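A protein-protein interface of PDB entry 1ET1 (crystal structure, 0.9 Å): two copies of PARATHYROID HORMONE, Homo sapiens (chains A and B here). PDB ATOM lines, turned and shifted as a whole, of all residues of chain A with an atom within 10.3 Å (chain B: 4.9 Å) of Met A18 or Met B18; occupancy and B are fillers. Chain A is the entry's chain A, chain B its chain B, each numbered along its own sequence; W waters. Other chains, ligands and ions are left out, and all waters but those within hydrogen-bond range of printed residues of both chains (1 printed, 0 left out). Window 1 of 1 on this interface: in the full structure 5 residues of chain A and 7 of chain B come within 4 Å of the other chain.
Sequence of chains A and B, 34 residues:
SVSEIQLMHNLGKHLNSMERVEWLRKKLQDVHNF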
ATOM      1  N   LEU A   7     -11.986  41.390 -19.879  1.00  0.00           N
ATOM      2  CA  LEU A   7     -11.528  40.083 -20.361  1.00  0.00           C
ATOM      3  C   LEU A   7     -10.120  39.825 -19.864  1.00  0.00           C
ATOM      4  O   LEU A   7      -9.796  38.710 -19.397  1.00  0.00           O
ATOM      5  CB  LEU A   7     -11.699  40.032 -21.874  1.00  0.00           C
ATOM      6  CG  LEU A   7     -11.418  38.621 -22.370  1.00  0.00           C
ATOM      7  CD1 LEU A   7     -12.346  38.311 -23.546  1.00  0.00           C
ATOM      8  CD2 LEU A   7      -9.974  38.418 -22.798  1.00  0.00           C
ATOM      9  N   MET A   8      -9.216  40.813 -19.966  1.00  0.00           N
ATOM     10  CA  MET A   8      -7.848  40.626 -19.497  1.00  0.00           C
ATOM     11  C   MET A   8      -7.797  40.398 -17.996  1.00  0.00           C
ATOM     12  O   MET A   8      -6.967  39.597 -17.533  1.00  0.00           O
ATOM     13  CB  MET A   8      -6.928  41.753 -19.944  1.00  0.00           C
ATOM     14  CG  MET A   8      -6.624  41.744 -21.450  1.00  0.00           C
ATOM     15  SD  MET A   8      -5.850  40.249 -22.071  1.00  0.00           S
ATOM     16  CE  MET A   8      -4.449  40.167 -21.008  1.00  0.00           C
ATOM     17  N   ASN A  10     -10.162  38.916 -16.146  1.00  0.00           N
ATOM     18  CA  ASN A  10     -10.617  37.547 -15.933  1.00  0.00           C
ATOM     19  C   ASN A  10      -9.566  36.550 -16.354  1.00  0.00           C
ATOM     20  O   ASN A  10      -9.336  35.532 -15.681  1.00  0.00           O
ATOM     21  CB  ASN A  10     -11.930  37.325 -16.677  1.00  0.00           C
ATOM     22  CG  ASN A  10     -13.102  38.092 -16.128  1.00  0.00           C
ATOM     23  OD1 ASN A  10     -14.146  38.247 -16.811  1.00  0.00           O
ATOM     24  ND2 ASN A  10     -13.101  38.563 -14.926  1.00  0.00           N
ATOM     25  N   LEU A  11      -8.925  36.820 -17.503  1.00  0.00           N
ATOM     26  CA  LEU A  11      -7.873  35.933 -17.986  1.00  0.00           C
ATOM     27  C   LEU A  11      -6.731  35.838 -16.986  1.00  0.00           C
ATOM     28  O   LEU A  11      -6.206  34.737 -16.715  1.00  0.00           O
ATOM     29  CB  LEU A  11      -7.432  36.377 -19.364  1.00  0.00           C
ATOM     30  CG  LEU A  11      -6.282  35.578 -19.988  1.00  0.00           C
ATOM     31  CD1 LEU A  11      -6.571  34.115 -20.090  1.00  0.00           C
ATOM     32  CD2 LEU A  11      -5.964  36.164 -21.361  1.00  0.00           C
ATOM     33  N   GLY A  12      -6.328  36.968 -16.433  1.00  0.00           N
ATOM     34  CA  GLY A  12      -5.219  36.920 -15.472  1.00  0.00           C
ATOM     35  C   GLY A  12      -5.609  36.126 -14.225  1.00  0.00           C
ATOM     36  O   GLY A  12      -4.779  35.403 -13.675  1.00  0.00           O
ATOM     37  N   LYS A  13      -6.850  36.279 -13.789  1.00  0.00           N
ATOM     38  CA  LYS A  13      -7.320  35.504 -12.649  1.00  0.00           C
ATOM     39  C   LYS A  13      -7.283  34.017 -12.970  1.00  0.00           C
ATOM     40  O   LYS A  13      -6.859  33.182 -12.140  1.00  0.00           O
ATOM     41  CB  LYS A  13      -8.714  35.996 -12.228  1.00  0.00           C
ATOM     42  CG  LYS A  13      -8.633  37.392 -11.587  1.00  0.00           C
ATOM     43  CD  LYS A  13     -10.029  37.984 -11.374  1.00  0.00           C
ATOM     44  CE  LYS A  13      -9.976  39.371 -10.727  1.00  0.00           C
ATOM     45  NZ  LYS A  13     -11.288  40.012 -10.678  1.00  0.00           N
ATOM     46  N   HIS A  14      -7.749  33.620 -14.168  1.00  0.00           N
ATOM     47  CA  HIS A  14      -7.709  32.211 -14.537  1.00  0.00           C
ATOM     48  C   HIS A  14      -6.284  31.689 -14.667  1.00  0.00           C
ATOM     49  O   HIS A  14      -6.014  30.532 -14.271  1.00  0.00           O
ATOM     50  CB  HIS A  14      -8.587  31.966 -15.766  1.00  0.00           C
ATOM     51  CG  HIS A  14     -10.005  32.381 -15.475  1.00  0.00           C
ATOM     52  ND1 HIS A  14     -10.902  32.786 -16.415  1.00  0.00           N
ATOM     53  CD2 HIS A  14     -10.644  32.550 -14.294  1.00  0.00           C
ATOM     54  CE1 HIS A  14     -12.059  33.109 -15.877  1.00  0.00           C
ATOM     55  NE2 HIS A  14     -11.920  32.968 -14.573  1.00  0.00           N
ATOM     56  N   LEU A  15      -5.370  32.474 -15.242  1.00  0.00           N
ATOM     57  CA  LEU A  15      -3.988  32.027 -15.346  1.00  0.00           C
ATOM     58  C   LEU A  15      -3.396  31.846 -13.945  1.00  0.00           C
ATOM     59  O   LEU A  15      -2.699  30.869 -13.693  1.00  0.00           O
ATOM     60  CB  LEU A  15      -3.166  33.017 -16.160  1.00  0.00           C
ATOM     61  CG  LEU A  15      -3.506  33.062 -17.653  1.00  0.00           C
ATOM     62  CD1 LEU A  15      -2.791  34.269 -18.302  1.00  0.00           C
ATOM     63  CD2 LEU A  15      -3.154  31.788 -18.360  1.00  0.00           C
ATOM     64  N   ASN A  16      -3.677  32.768 -13.036  1.00  0.00           N
ATOM     65  CA  ASN A  16      -3.236  32.602 -11.651  1.00  0.00           C
ATOM     66  C   ASN A  16      -3.746  31.314 -11.025  1.00  0.00           C
ATOM     67  O   ASN A  16      -3.007  30.600 -10.342  1.00  0.00           O
ATOM     68  CB  ASN A  16      -3.613  33.813 -10.810  1.00  0.00           C
ATOM     69  CG  ASN A  16      -2.735  35.052 -10.943  1.00  0.00           C
ATOM     70  OD1 ASN A  16      -3.057  36.069 -10.245  1.00  0.00           O
ATOM     71  ND2 ASN A  16      -1.702  35.040 -11.703  1.00  0.00           N
ATOM     72  N   SER A  17      -5.010  30.994 -11.275  1.00  0.00           N
ATOM     73  CA  SER A  17      -5.533  29.740 -10.749  1.00  0.00           C
ATOM     74  C   SER A  17      -4.805  28.528 -11.342  1.00  0.00           C
ATOM     75  O   SER A  17      -4.501  27.538 -10.651  1.00  0.00           O
ATOM     76  CB  SER A  17      -7.044  29.667 -11.031  1.00  0.00           C
ATOM     77  OG  SER A  17      -7.765  30.685 -10.364  1.00  0.00           O
ATOM     78  N   MET A  18      -4.499  28.577 -12.638  1.00  0.00           N
ATOM     79  CA  MET A  18      -3.766  27.475 -13.275  1.00  0.00           C
ATOM     80  C   MET A  18      -2.351  27.363 -12.718  1.00  0.00           C
ATOM     81  O   MET A  18      -1.868  26.229 -12.590  1.00  0.00           O
ATOM     82  CB  MET A  18      -3.697  27.715 -14.789  1.00  0.00           C
ATOM     83  CG  MET A  18      -4.984  27.685 -15.582  1.00  0.00           C
ATOM     84  SD  MET A  18      -5.845  26.129 -15.359  1.00  0.00           S
ATOM     85  CE  MET A  18      -4.869  25.038 -16.385  1.00  0.00           C
ATOM     86  N   GLU A  19      -1.718  28.494 -12.377  1.00  0.00           N
ATOM     87  CA  GLU A  19      -0.411  28.420 -11.730  1.00  0.00           C
ATOM     88  C   GLU A  19      -0.504  27.640 -10.429  1.00  0.00           C
ATOM     89  O   GLU A  19       0.382  26.827 -10.100  1.00  0.00           O
ATOM     90  CB  GLU A  19       0.116  29.824 -11.437  1.00  0.00           C
ATOM     91  CG  GLU A  19       0.450  30.656 -12.678  1.00  0.00           C
ATOM     92  CD  GLU A  19       0.643  32.127 -12.298  1.00  0.00           C
ATOM     93  OE1 GLU A  19       1.118  32.391 -11.184  1.00  0.00           O
ATOM     94  OE2 GLU A  19       0.369  32.986 -13.129  1.00  0.00           O
ATOM     95  N   ARG A  20      -1.575  27.885  -9.668  1.00  0.00           N
ATOM     96  CA  ARG A  20      -1.759  27.166  -8.387  1.00  0.00           C
ATOM     97  C   ARG A  20      -2.005  25.689  -8.605  1.00  0.00           C
ATOM     98  O   ARG A  20      -1.534  24.846  -7.829  1.00  0.00           O
ATOM     99  CB  ARG A  20      -2.857  27.841  -7.557  1.00  0.00           C
ATOM    100  CG  ARG A  20      -2.429  29.247  -7.115  1.00  0.00           C
ATOM    101  CD  ARG A  20      -3.269  29.931  -6.102  1.00  0.00           C
ATOM    102  NE  ARG A  20      -4.457  30.467  -6.679  1.00  0.00           N
ATOM    103  CZ  ARG A  20      -5.642  29.925  -6.746  1.00  0.00           C
ATOM    104  NH1 ARG A  20      -5.875  28.744  -6.257  1.00  0.00           N
ATOM    105  NH2 ARG A  20      -6.655  30.545  -7.333  1.00  0.00           N
ATOM    106  N   VAL A  21      -2.775  25.342  -9.636  1.00  0.00           N
ATOM    107  CA  VAL A  21      -2.997  23.926  -9.923  1.00  0.00           C
ATOM    108  C   VAL A  21      -1.686  23.265 -10.325  1.00  0.00           C
ATOM    109  O   VAL A  21      -1.428  22.107  -9.953  1.00  0.00           O
ATOM    110  CB  VAL A  21      -4.087  23.785 -10.979  1.00  0.00           C
ATOM    111  CG1 VAL A  21      -4.204  22.324 -11.396  1.00  0.00           C
ATOM    112  CG2 VAL A  21      -5.407  24.309 -10.469  1.00  0.00           C
ATOM    113  N   GLU A  22      -0.829  23.962 -11.100  1.00  0.00           N
ATOM    114  CA  GLU A  22       0.480  23.416 -11.484  1.00  0.00           C
ATOM    115  C   GLU A  22       1.421  23.330 -10.293  1.00  0.00           C
ATOM    116  O   GLU A  22       2.214  22.350 -10.193  1.00  0.00           O
ATOM    117  CB  GLU A  22       1.040  24.299 -12.614  1.00  0.00           C
ATOM    118  CG  GLU A  22       2.451  23.934 -13.035  1.00  0.00           C
ATOM    119  CD  GLU A  22       2.541  22.583 -13.709  1.00  0.00           C
ATOM    120  OE1 GLU A  22       3.675  22.265 -14.051  1.00  0.00           O
ATOM    121  OE2 GLU A  22       1.520  21.935 -13.881  1.00  0.00           O
ATOM    122  N   TRP A  23       1.356  24.278  -9.378  1.00  0.00           N
ATOM    123  CA  TRP A  23       2.059  24.170  -8.109  1.00  0.00           C
ATOM    124  C   TRP A  23       1.691  22.838  -7.407  1.00  0.00           C
ATOM    125  O   TRP A  23       2.554  22.074  -6.981  1.00  0.00           O
ATOM    126  CB  TRP A  23       1.712  25.367  -7.188  1.00  0.00           C
ATOM    127  CG  TRP A  23       2.219  25.206  -5.804  1.00  0.00           C
ATOM    128  CD1 TRP A  23       3.485  25.468  -5.390  1.00  0.00           C
ATOM    129  CD2 TRP A  23       1.505  24.743  -4.647  1.00  0.00           C
ATOM    130  NE1 TRP A  23       3.628  25.197  -4.040  1.00  0.00           N
ATOM    131  CE2 TRP A  23       2.406  24.750  -3.559  1.00  0.00           C
ATOM    132  CE3 TRP A  23       0.175  24.327  -4.417  1.00  0.00           C
ATOM    133  CZ2 TRP A  23       2.012  24.362  -2.284  1.00  0.00           C
ATOM    134  CZ3 TRP A  23      -0.188  23.930  -3.129  1.00  0.00           C
ATOM    135  CH2 TRP A  23       0.742  23.943  -2.078  1.00  0.00           C
ATOM    136  N   LEU A  24       0.384  22.592  -7.312  1.00  0.00           N
ATOM    137  CA  LEU A  24      -0.087  21.355  -6.665  1.00  0.00           C
ATOM    138  C   LEU A  24       0.420  20.147  -7.444  1.00  0.00           C
ATOM    139  O   LEU A  24       0.860  19.160  -6.833  1.00  0.00           O
ATOM    140  CB  LEU A  24      -1.611  21.361  -6.561  1.00  0.00           C
ATOM    141  CG  LEU A  24      -2.180  20.090  -5.950  1.00  0.00           C
ATOM    142  CD1 LEU A  24      -1.739  19.886  -4.515  1.00  0.00           C
ATOM    143  CD2 LEU A  24      -3.695  20.124  -6.013  1.00  0.00           C
ATOM    144  N   ARG A  25       0.285  20.174  -8.763  1.00  0.00           N
ATOM    145  CA  ARG A  25       0.733  19.026  -9.568  1.00  0.00           C
ATOM    146  C   ARG A  25       2.160  18.651  -9.224  1.00  0.00           C
ATOM    147  O   ARG A  25       2.497  17.460  -9.035  1.00  0.00           O
ATOM    148  CB  ARG A  25       0.585  19.306 -11.061  1.00  0.00           C
ATOM    149  CG  ARG A  25       0.959  18.107 -11.930  1.00  0.00           C
ATOM    150  CD  ARG A  25       0.968  18.395 -13.429  1.00  0.00           C
ATOM    151  NE  ARG A  25       1.977  19.314 -13.857  1.00  0.00           N
ATOM    152  CZ  ARG A  25       3.275  19.015 -14.077  1.00  0.00           C
ATOM    153  NH1 ARG A  25       3.692  17.772 -13.868  1.00  0.00           N
ATOM    154  NH2 ARG A  25       4.116  19.918 -14.475  1.00  0.00           N
ATOM    155  N   LYS A  26       3.059  19.658  -9.182  1.00  0.00           N
ATOM    156  CA  LYS A  26       4.471  19.370  -8.890  1.00  0.00           C
ATOM    157  C   LYS A  26       4.676  18.872  -7.482  1.00  0.00           C
ATOM    158  O   LYS A  26       5.544  18.006  -7.245  1.00  0.00           O
ATOM    159  CB  LYS A  26       5.326  20.560  -9.264  1.00  0.00           C
ATOM    160  CG  LYS A  26       5.415  20.772 -10.788  1.00  0.00           C
ATOM    161  CD  LYS A  26       6.432  21.809 -11.224  1.00  0.00           C
ATOM    162  CE  LYS A  26       6.180  22.360 -12.628  1.00  0.00           C
ATOM    163  NZ  LYS A  26       7.274  23.242 -13.095  1.00  0.00           N
ATOM    164  N   LEU B  11     -11.099  23.609 -11.885  1.00  0.00           N
ATOM    165  CA  LEU B  11     -10.185  23.477 -13.018  1.00  0.00           C
ATOM    166  C   LEU B  11     -10.952  23.389 -14.324  1.00  0.00           C
ATOM    167  O   LEU B  11     -10.596  24.015 -15.321  1.00  0.00           O
ATOM    168  CB  LEU B  11      -9.244  22.300 -12.800  1.00  0.00           C
ATOM    169  CG  LEU B  11      -8.263  22.005 -13.912  1.00  0.00           C
ATOM    170  CD1 LEU B  11      -7.412  23.202 -14.251  1.00  0.00           C
ATOM    171  CD2 LEU B  11      -7.427  20.803 -13.520  1.00  0.00           C
ATOM    172  N   HIS B  14     -12.201  26.755 -15.250  1.00  0.00           N
ATOM    173  CA  HIS B  14     -11.138  27.602 -15.787  1.00  0.00           C
ATOM    174  C   HIS B  14     -10.745  27.178 -17.193  1.00  0.00           C
ATOM    175  O   HIS B  14     -10.467  28.044 -18.071  1.00  0.00           O
ATOM    176  CB  HIS B  14      -9.889  27.473 -14.911  1.00  0.00           C
ATOM    177  CG  HIS B  14     -10.039  28.150 -13.582  1.00  0.00           C
ATOM    178  ND1 HIS B  14     -10.076  27.575 -12.351  1.00  0.00           N
ATOM    179  CD2 HIS B  14     -10.219  29.449 -13.367  1.00  0.00           C
ATOM    180  CE1 HIS B  14     -10.242  28.511 -11.413  1.00  0.00           C
ATOM    181  NE2 HIS B  14     -10.342  29.683 -12.000  1.00  0.00           N
ATOM    182  N   LEU B  15     -10.639  25.883 -17.449  1.00  0.00           N
ATOM    183  CA  LEU B  15     -10.302  25.420 -18.796  1.00  0.00           C
ATOM    184  C   LEU B  15     -11.372  25.873 -19.778  1.00  0.00           C
ATOM    185  O   LEU B  15     -11.048  26.314 -20.895  1.00  0.00           O
ATOM    186  CB  LEU B  15     -10.113  23.896 -18.828  1.00  0.00           C
ATOM    187  CG  LEU B  15      -8.865  23.396 -18.082  1.00  0.00           C
ATOM    188  CD1 LEU B  15      -8.907  21.893 -17.921  1.00  0.00           C
ATOM    189  CD2 LEU B  15      -7.588  23.837 -18.773  1.00  0.00           C
ATOM    190  N   ASN B  16     -12.639  25.746 -19.408  1.00  0.00           N
ATOM    191  CA  ASN B  16     -13.726  26.224 -20.278  1.00  0.00           C
ATOM    192  C   ASN B  16     -13.587  27.716 -20.586  1.00  0.00           C
ATOM    193  O   ASN B  16     -13.783  28.141 -21.730  1.00  0.00           O
ATOM    194  CB  ASN B  16     -15.084  25.913 -19.668  1.00  0.00           C
ATOM    195  CG  ASN B  16     -15.564  24.480 -19.851  1.00  0.00           C
ATOM    196  OD1 ASN B  16     -14.906  23.633 -20.482  1.00  0.00           O
ATOM    197  ND2 ASN B  16     -16.737  24.257 -19.311  1.00  0.00           N
ATOM    198  N   SER B  17     -13.212  28.535 -19.586  1.00  0.00           N
ATOM    199  CA  SER B  17     -13.009  29.945 -19.837  1.00  0.00           C
ATOM    200  C   SER B  17     -11.872  30.158 -20.829  1.00  0.00           C
ATOM    201  O   SER B  17     -11.941  31.005 -21.725  1.00  0.00           O
ATOM    202  CB  SER B  17     -12.622  30.658 -18.517  1.00  0.00           C
ATOM    203  OG  SER B  17     -11.293  30.424 -18.090  1.00  0.00           O
ATOM    204  N   MET B  18     -10.777  29.395 -20.668  1.00  0.00           N
ATOM    205  CA  MET B  18      -9.649  29.521 -21.577  1.00  0.00           C
ATOM    206  C   MET B  18     -10.019  29.092 -23.008  1.00  0.00           C
ATOM    207  O   MET B  18      -9.513  29.723 -23.968  1.00  0.00           O
ATOM    208  CB  MET B  18      -8.441  28.812 -20.964  1.00  0.00           C
ATOM    209  CG  MET B  18      -8.109  29.621 -19.700  1.00  0.00           C
ATOM    210  SD  MET B  18      -6.665  28.904 -18.926  1.00  0.00           S
ATOM    211  CE  MET B  18      -6.700  27.257 -19.605  1.00  0.00           C
ATOM    212  N   GLU B  19     -10.892  28.090 -23.152  1.00  0.00           N
ATOM    213  CA  GLU B  19     -11.383  27.753 -24.480  1.00  0.00           C
ATOM    214  C   GLU B  19     -12.075  28.947 -25.124  1.00  0.00           C
ATOM    215  O   GLU B  19     -11.919  29.201 -26.347  1.00  0.00           O
ATOM    216  CB  GLU B  19     -12.366  26.570 -24.407  1.00  0.00           C
ATOM    217  CG  GLU B  19     -11.762  25.252 -23.962  1.00  0.00           C
ATOM    218  CD  GLU B  19     -12.832  24.256 -23.582  1.00  0.00           C
ATOM    219  OE1 GLU B  19     -13.927  24.299 -24.188  1.00  0.00           O
ATOM    220  OE2 GLU B  19     -12.606  23.412 -22.694  1.00  0.00           O
ATOM    221  N   ARG B  20     -12.871  29.667 -24.340  1.00  0.00           N
ATOM    222  CA  ARG B  20     -13.590  30.827 -24.893  1.00  0.00           C
ATOM    223  C   ARG B  20     -12.628  31.946 -25.254  1.00  0.00           C
ATOM    224  O   ARG B  20     -12.850  32.645 -26.253  1.00  0.00           O
ATOM    225  CB  ARG B  20     -14.655  31.291 -23.898  1.00  0.00           C
ATOM    226  CG  ARG B  20     -15.780  30.235 -23.791  1.00  0.00           C
ATOM    227  CD  ARG B  20     -17.017  30.662 -23.079  1.00  0.00           C
ATOM    228  NE  ARG B  20     -16.843  30.651 -21.668  1.00  0.00           N
ATOM    229  CZ  ARG B  20     -16.516  31.613 -20.860  1.00  0.00           C
ATOM    230  NH1 ARG B  20     -16.244  32.804 -21.348  1.00  0.00           N
ATOM    231  NH2 ARG B  20     -16.444  31.304 -19.574  1.00  0.00           N
ATOM    232  N   VAL B  21     -11.592  32.162 -24.445  1.00  0.00           N
ATOM    233  CA  VAL B  21     -10.609  33.172 -24.799  1.00  0.00           C
ATOM    234  C   VAL B  21      -9.886  32.787 -26.090  1.00  0.00           C
ATOM    235  O   VAL B  21      -9.589  33.644 -26.933  1.00  0.00           O
ATOM    236  CB  VAL B  21      -9.632  33.405 -23.641  1.00  0.00           C
ATOM    237  CG1 VAL B  21      -8.503  34.325 -24.056  1.00  0.00           C
ATOM    238  CG2 VAL B  21     -10.371  33.911 -22.427  1.00  0.00           C
ATOM    239  N   GLU B  22      -9.573  31.491 -26.275  1.00  0.00           N
ATOM    240  CA  GLU B  22      -8.934  31.017 -27.518  1.00  0.00           C
ATOM    241  C   GLU B  22      -9.891  31.103 -28.703  1.00  0.00           C
ATOM    242  O   GLU B  22      -9.449  31.442 -29.826  1.00  0.00           O
ATOM    243  CB  GLU B  22      -8.447  29.576 -27.302  1.00  0.00           C
ATOM    244  CG  GLU B  22      -7.852  28.920 -28.542  1.00  0.00           C
ATOM    245  CD  GLU B  22      -6.526  29.508 -28.929  1.00  0.00           C
ATOM    246  OE1 GLU B  22      -6.077  30.518 -28.365  1.00  0.00           O
ATOM    247  OE2 GLU B  22      -5.952  28.871 -29.821  1.00  0.00           O
HETATM  248  O   HOH W   1     -10.110  32.213 -10.921  1.00  0.00           O
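O of Asn A10 lies close to ND1 of His A14 (3.2 Å).
O of Lys A13 sits at hydrogen-bond distance from OG of Ser A17 (3.2 Å).
The side-chain hydroxyl of Ser A17 is in hydrogen-bond range of the guanidinium group of Arg A20, 3.2 Å away.
The side-chain hydroxyl of Ser B17 sits at hydrogen-bond distance from the backbone carbonyl oxygen of His B14, at 2.5 Å.
Of the 10 printed residues of chain B, 5 touch a printed residue of chain A.
Printed residues of chain B that touch a printed residue of chain A: Leu B11, His B14, Leu B15, Ser B17 and Met B18.
Among the printed residues, no Asp or Glu carboxylate lies within 4 Å of a Lys or Arg side-chain nitrogen of the other chain.
A ring nitrogen (ND1) of His A14 sits at hydrogen-bond distance from the side-chain hydroxyl (OG) of Ser B17.
The side-chain hydroxyl (OG) of Ser A17 lies within hydrogen-bond range of a ring nitrogen (NE2) of His B14.
His B14 touches its own counterpart, His A14.
His A14 touches Ser B17, and with the chains exchanged Ser A17 touches His B14.
Met A18 touches Leu B11, but with the chains exchanged Leu A11 does not touch Met B18 (4.8 Å).
Met A18 touches Leu B15, but with the chains exchanged Leu A15 does not touch Met B18 (4.6 Å).
Positions printed for both chains: 11, 14, 15, 16, 17, 18, 19, 20, 21 and 22.
Of the 6 pairs that touch across the chains among the printed residues, 4 have their exchanged pair printed and touching as well.
Among the printed residues, merely in contact across the chains: His A14 with His B14 (3.3 Å), Met A18 with Leu B11 (3.5 Å), Met A18 with Leu B15 (3.8 Å) and Met A18 with Met B18 (3.9 Å).
Water W1 lies within hydrogen-bond range of NE2 of His B14 (2.8 Å) and OG of Ser A17 (2.9 Å).
Printed residues of chain B within 4 Å of Ser A17: His B14 (3.2 Å).
Of the printed residues of chain B, Met A18 touches Leu B11, Leu B15 and Met B18.
Printed residues of chain A within 4 Å of Leu B11: Met A18.
Printed residues of chain A within 4 Å of Met B18: Met A18.
Val B21 touches none of the printed residues of chain A.
The nearest printed residue of chain A that does not touch Leu B11 is Val A21 (4.1 Å).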
